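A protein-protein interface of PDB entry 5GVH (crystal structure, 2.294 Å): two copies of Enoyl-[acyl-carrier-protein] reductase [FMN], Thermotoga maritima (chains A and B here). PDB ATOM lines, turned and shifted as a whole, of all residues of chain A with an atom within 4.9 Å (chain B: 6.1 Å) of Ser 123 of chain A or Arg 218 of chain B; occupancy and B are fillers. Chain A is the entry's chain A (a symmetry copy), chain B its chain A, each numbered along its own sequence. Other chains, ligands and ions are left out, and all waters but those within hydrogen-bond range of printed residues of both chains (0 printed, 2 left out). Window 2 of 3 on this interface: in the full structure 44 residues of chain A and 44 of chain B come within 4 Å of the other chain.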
ATOM      1  N   SER A 121      10.165   4.778 -11.407  1.00  0.00           N
ATOM      2  CA  SER A 121      11.090   3.693 -11.125  1.00  0.00           C
ATOM      3  C   SER A 121      12.183   3.731 -12.180  1.00  0.00           C
ATOM      4  O   SER A 121      11.978   4.228 -13.296  1.00  0.00           O
ATOM      5  CB  SER A 121      10.381   2.334 -11.126  1.00  0.00           C
ATOM      6  OG  SER A 121       9.820   2.045 -12.405  1.00  0.00           O
ATOM      7  N   ASP A 122      13.350   3.204 -11.814  1.00  0.00           N
ATOM      8  CA  ASP A 122      14.446   3.123 -12.774  1.00  0.00           C
ATOM      9  C   ASP A 122      14.159   2.086 -13.855  1.00  0.00           C
ATOM     10  O   ASP A 122      14.497   2.298 -15.029  1.00  0.00           O
ATOM     11  CB  ASP A 122      15.764   2.820 -12.053  1.00  0.00           C
ATOM     12  CG  ASP A 122      15.704   1.555 -11.208  1.00  0.00           C
ATOM     13  OD1 ASP A 122      14.698   1.358 -10.486  1.00  0.00           O
ATOM     14  OD2 ASP A 122      16.684   0.773 -11.248  1.00  0.00           O
ATOM     15  N   SER A 123      13.524   0.970 -13.486  1.00  0.00           N
ATOM     16  CA  SER A 123      13.263  -0.086 -14.461  1.00  0.00           C
ATOM     17  C   SER A 123      12.312   0.388 -15.550  1.00  0.00           C
ATOM     18  O   SER A 123      12.480   0.032 -16.721  1.00  0.00           O
ATOM     19  CB  SER A 123      12.722  -1.334 -13.759  1.00  0.00           C
ATOM     20  OG  SER A 123      11.570  -1.037 -12.983  1.00  0.00           O
ATOM     21  N   LEU A 124      11.320   1.207 -15.193  1.00  0.00           N
ATOM     22  CA  LEU A 124      10.455   1.786 -16.216  1.00  0.00           C
ATOM     23  C   LEU A 124      11.146   2.920 -16.960  1.00  0.00           C
ATOM     24  O   LEU A 124      10.909   3.095 -18.159  1.00  0.00           O
ATOM     25  CB  LEU A 124       9.146   2.286 -15.596  1.00  0.00           C
ATOM     26  CG  LEU A 124       8.082   2.879 -16.528  1.00  0.00           C
ATOM     27  CD1 LEU A 124       7.839   2.012 -17.762  1.00  0.00           C
ATOM     28  CD2 LEU A 124       6.786   3.095 -15.776  1.00  0.00           C
ATOM     29  N   ALA A 125      11.989   3.695 -16.267  1.00  0.00           N
ATOM     30  CA  ALA A 125      12.761   4.742 -16.931  1.00  0.00           C
ATOM     31  C   ALA A 125      13.619   4.155 -18.035  1.00  0.00           C
ATOM     32  O   ALA A 125      13.649   4.670 -19.160  1.00  0.00           O
ATOM     33  CB  ALA A 125      13.640   5.480 -15.915  1.00  0.00           C
ATOM     34  N   ARG A 126      14.308   3.061 -17.729  1.00  0.00           N
ATOM     35  CA  ARG A 126      15.169   2.396 -18.698  1.00  0.00           C
ATOM     36  C   ARG A 126      14.352   1.714 -19.793  1.00  0.00           C
ATOM     37  O   ARG A 126      14.767   1.680 -20.958  1.00  0.00           O
ATOM     38  CB  ARG A 126      16.056   1.397 -17.956  1.00  0.00           C
ATOM     39  CG  ARG A 126      16.738   0.392 -18.837  1.00  0.00           C
ATOM     40  CD  ARG A 126      17.762   1.081 -19.762  1.00  0.00           C
ATOM     41  NE  ARG A 126      18.603   0.083 -20.393  1.00  0.00           N
ATOM     42  CZ  ARG A 126      19.140   0.212 -21.600  1.00  0.00           C
ATOM     43  NH1 ARG A 126      18.935   1.309 -22.330  1.00  0.00           N
ATOM     44  NH2 ARG A 126      19.890  -0.766 -22.093  1.00  0.00           N
ATOM     45  N   MET A 127      13.182   1.174 -19.437  1.00  0.00           N
ATOM     46  CA  MET A 127      12.328   0.507 -20.415  1.00  0.00           C
ATOM     47  C   MET A 127      11.848   1.483 -21.486  1.00  0.00           C
ATOM     48  O   MET A 127      11.776   1.131 -22.668  1.00  0.00           O
ATOM     49  CB  MET A 127      11.135  -0.139 -19.702  1.00  0.00           C
ATOM     50  CG  MET A 127      10.875  -1.605 -20.034  1.00  0.00           C
ATOM     51  SD  MET A 127       9.771  -2.376 -18.815  1.00  0.00           S
ATOM     52  CE  MET A 127       8.227  -1.510 -19.133  1.00  0.00           C
ATOM     53  N   GLU A 149       5.951   5.409  -5.493  1.00  0.00           N
ATOM     54  CA  GLU A 149       6.352   4.919  -4.179  1.00  0.00           C
ATOM     55  C   GLU A 149       7.736   5.385  -3.754  1.00  0.00           C
ATOM     56  O   GLU A 149       8.143   5.117  -2.624  1.00  0.00           O
ATOM     57  CB  GLU A 149       6.319   3.385  -4.143  1.00  0.00           C
ATOM     58  CG  GLU A 149       4.928   2.763  -4.255  1.00  0.00           C
ATOM     59  CD  GLU A 149       4.936   1.266  -3.943  1.00  0.00           C
ATOM     60  OE1 GLU A 149       5.998   0.755  -3.512  1.00  0.00           O
ATOM     61  OE2 GLU A 149       3.878   0.613  -4.111  1.00  0.00           O
ATOM     62  N   VAL A 150       8.475   6.058  -4.614  1.00  0.00           N
ATOM     63  CA  VAL A 150       9.815   6.526  -4.300  1.00  0.00           C
ATOM     64  C   VAL A 150       9.771   8.039  -4.161  1.00  0.00           C
ATOM     65  O   VAL A 150       9.005   8.709  -4.864  1.00  0.00           O
ATOM     66  CB  VAL A 150      10.806   6.067  -5.390  1.00  0.00           C
ATOM     67  CG1 VAL A 150      12.228   6.484  -5.057  1.00  0.00           C
ATOM     68  CG2 VAL A 150      10.734   4.550  -5.528  1.00  0.00           C
ATOM     69  N   ALA B 215      18.546  -4.808  -2.507  1.00  0.00           N
ATOM     70  CA  ALA B 215      17.261  -4.125  -2.480  1.00  0.00           C
ATOM     71  C   ALA B 215      17.275  -2.968  -3.465  1.00  0.00           C
ATOM     72  O   ALA B 215      18.274  -2.253  -3.596  1.00  0.00           O
ATOM     73  CB  ALA B 215      16.924  -3.622  -1.072  1.00  0.00           C
ATOM     74  N   SER B 216      16.176  -2.815  -4.191  1.00  0.00           N
ATOM     75  CA  SER B 216      15.993  -1.665  -5.057  1.00  0.00           C
ATOM     76  C   SER B 216      15.378  -0.522  -4.255  1.00  0.00           C
ATOM     77  O   SER B 216      15.088  -0.649  -3.064  1.00  0.00           O
ATOM     78  CB  SER B 216      15.108  -2.029  -6.242  1.00  0.00           C
ATOM     79  OG  SER B 216      13.816  -2.357  -5.769  1.00  0.00           O
ATOM     80  N   ILE B 217      15.163   0.616  -4.915  1.00  0.00           N
ATOM     81  CA  ILE B 217      14.484   1.727  -4.263  1.00  0.00           C
ATOM     82  C   ILE B 217      13.000   1.477  -4.064  1.00  0.00           C
ATOM     83  O   ILE B 217      12.357   2.233  -3.331  1.00  0.00           O
ATOM     84  CB  ILE B 217      14.720   3.011  -5.071  1.00  0.00           C
ATOM     85  CG1 ILE B 217      14.108   2.883  -6.477  1.00  0.00           C
ATOM     86  CG2 ILE B 217      16.198   3.274  -5.162  1.00  0.00           C
ATOM     87  CD1 ILE B 217      14.404   4.068  -7.368  1.00  0.00           C
ATOM     88  N   ARG B 218      12.445   0.421  -4.672  1.00  0.00           N
ATOM     89  CA  ARG B 218      11.050   0.032  -4.470  1.00  0.00           C
ATOM     90  C   ARG B 218      10.860  -1.044  -3.409  1.00  0.00           C
ATOM     91  O   ARG B 218       9.710  -1.350  -3.062  1.00  0.00           O
ATOM     92  CB  ARG B 218      10.444  -0.472  -5.783  1.00  0.00           C
ATOM     93  CG  ARG B 218      10.081   0.621  -6.741  1.00  0.00           C
ATOM     94  CD  ARG B 218       9.528   0.045  -8.029  1.00  0.00           C
ATOM     95  NE  ARG B 218      10.571  -0.501  -8.892  1.00  0.00           N
ATOM     96  CZ  ARG B 218      10.333  -1.035 -10.087  1.00  0.00           C
ATOM     97  NH1 ARG B 218       9.092  -1.094 -10.555  1.00  0.00           N
ATOM     98  NH2 ARG B 218      11.333  -1.501 -10.821  1.00  0.00           N
ATOM     99  N   ASP B 219      11.946  -1.621  -2.886  1.00  0.00           N
ATOM    100  CA  ASP B 219      11.886  -2.798  -2.026  1.00  0.00           C
ATOM    101  C   ASP B 219      11.679  -2.453  -0.555  1.00  0.00           C
ATOM    102  O   ASP B 219      12.207  -3.153   0.322  1.00  0.00           O
ATOM    103  CB  ASP B 219      13.153  -3.644  -2.198  1.00  0.00           C
ATOM    104  CG  ASP B 219      13.189  -4.399  -3.529  1.00  0.00           C
ATOM    105  OD1 ASP B 219      12.121  -4.837  -4.016  1.00  0.00           O
ATOM    106  OD2 ASP B 219      14.297  -4.555  -4.091  1.00  0.00           O
ATOM    107  N   THR B 220      10.939  -1.391  -0.249  1.00  0.00           N
ATOM    108  CA  THR B 220      10.565  -1.103   1.125  1.00  0.00           C
ATOM    109  C   THR B 220       9.065  -0.855   1.192  1.00  0.00           C
ATOM    110  O   THR B 220       8.425  -0.552   0.187  1.00  0.00           O
ATOM    111  CB  THR B 220      11.326   0.106   1.712  1.00  0.00           C
ATOM    112  OG1 THR B 220      10.667   1.323   1.355  1.00  0.00           O
ATOM    113  CG2 THR B 220      12.773   0.136   1.220  1.00  0.00           C
ATOM    114  N   VAL B 221       8.511  -1.033   2.392  1.00  0.00           N
ATOM    115  CA  VAL B 221       7.106  -0.781   2.692  1.00  0.00           C
ATOM    116  C   VAL B 221       7.050  -0.182   4.089  1.00  0.00           C
ATOM    117  O   VAL B 221       8.003  -0.267   4.863  1.00  0.00           O
ATOM    118  CB  VAL B 221       6.234  -2.057   2.636  1.00  0.00           C
ATOM    119  CG1 VAL B 221       6.162  -2.601   1.225  1.00  0.00           C
ATOM    120  CG2 VAL B 221       6.777  -3.110   3.590  1.00  0.00           C
ATOM    121  N   ARG B 235      10.760  -4.804   2.084  1.00  0.00           N
ATOM    122  CA  ARG B 235       9.557  -5.415   1.542  1.00  0.00           C
ATOM    123  C   ARG B 235       9.670  -6.928   1.629  1.00  0.00           C
ATOM    124  O   ARG B 235      10.420  -7.554   0.872  1.00  0.00           O
ATOM    125  CB  ARG B 235       9.328  -4.973   0.092  1.00  0.00           C
ATOM    126  CG  ARG B 235       7.973  -5.337  -0.441  1.00  0.00           C
ATOM    127  CD  ARG B 235       7.828  -4.900  -1.882  1.00  0.00           C
ATOM    128  NE  ARG B 235       6.543  -4.249  -2.087  1.00  0.00           N
ATOM    129  CZ  ARG B 235       6.384  -2.938  -2.221  1.00  0.00           C
ATOM    130  NH1 ARG B 235       7.441  -2.135  -2.197  1.00  0.00           N
ATOM    131  NH2 ARG B 235       5.169  -2.437  -2.392  1.00  0.00           N
ATOM    132  N   GLN B 279      14.625   3.895   1.690  1.00  0.00           N
ATOM    133  CA  GLN B 279      14.670   3.777   0.237  1.00  0.00           C
ATOM    134  C   GLN B 279      16.085   3.927  -0.305  1.00  0.00           C
ATOM    135  O   GLN B 279      16.360   3.470  -1.422  1.00  0.00           O
ATOM    136  CB  GLN B 279      13.754   4.818  -0.405  1.00  0.00           C
ATOM    137  CG  GLN B 279      12.319   4.688   0.037  1.00  0.00           C
ATOM    138  CD  GLN B 279      11.364   5.515  -0.795  1.00  0.00           C
ATOM    139  OE1 GLN B 279      11.758   6.497  -1.419  1.00  0.00           O
ATOM    140  NE2 GLN B 279      10.099   5.105  -0.829  1.00  0.00           N
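No position is printed for both chains.
N of Arg 235 of chain B lies within hydrogen-bond range of O of Asp 219 of chain B (2.8 Å).
OG of Ser 121 of chain A sits close to N of Leu 124 of chain A (3.3 Å).
The backbone carbonyl oxygen of Thr 220 of chain B sits at hydrogen-bond distance from the guanidinium group of Arg 235 of chain B.
The side-chain hydroxyl (OG) of Ser 216 of chain B sits close to the backbone NH (N) of Arg 218 of chain B (3.3 Å).
NH1 of Arg 235 of chain B sits at hydrogen-bond distance from O of Arg 218 of chain B, 2.6 Å away.
Hydrophobic or aromatic side chains of chain A that line the printed part of chain B: Val 150.
Along chain A the printed residues that touch a printed residue of chain B span positions 121 to 150.
Hydrophobic or aromatic side chains of chain B within 4 Å of the printed part of chain A: Ile 217.
Ser 121 of chain A touches Arg 218 of chain B (CB to CZ, 3.5 Å).
Ile 217 of chain B touches Val 150 of chain A (O to CG2, 3.6 Å).
Gln 279 of chain B touches Val 150 of chain A (OE1 to CA, 3.5 Å).
Ser 123 of chain A touches just one residue of chain B: Arg 218.
Of chain A, only Ser 121 and Ser 123 come within 4 Å of Arg 218 of chain B.
Printed residues of chain B within 4 Å of Ser 121 of chain A: Arg 218 (3.5 Å).
Of the printed residues of chain A, Arg 235 of chain B touches Glu 149 (3.5 Å).
Of the printed residues of chain A, Gln 279 of chain B touches Glu 149 (2.7 Å) and Val 150 (3.5 Å).
Of the printed residues of chain B, Glu 149 of chain A touches Arg 235 (3.5 Å) and Gln 279 (2.7 Å).
Of the printed residues of chain A, Ile 217 of chain B touches Val 150 (3.6 Å).
The nearest printed residue of chain B that does not touch Ser 123 of chain A is Ile 217 of chain B (6.9 Å).
The nearest residue of chain A that does not touch Arg 218 of chain B is Val 150 of chain A (4.2 Å).
The nearest printed residue of chain A that does not touch Ile 217 of chain B is Asp 122 of chain A (4.1 Å).
The backbone carbonyl oxygen (O) of Glu 149 of chain A is in hydrogen-bond range of the side-chain amide nitrogen (NE2) of Gln 279 of chain B (2.7 Å).
The side-chain carboxylate (OE1) of Glu 149 of chain A is in salt-bridge range of the guanidinium group (NH2) of Arg 235 of chain B (3.5 Å).
The guanidinium group of Arg 218 of chain B sits close to the side-chain hydroxyl of Ser 123 of chain A, 3.5 Å away.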
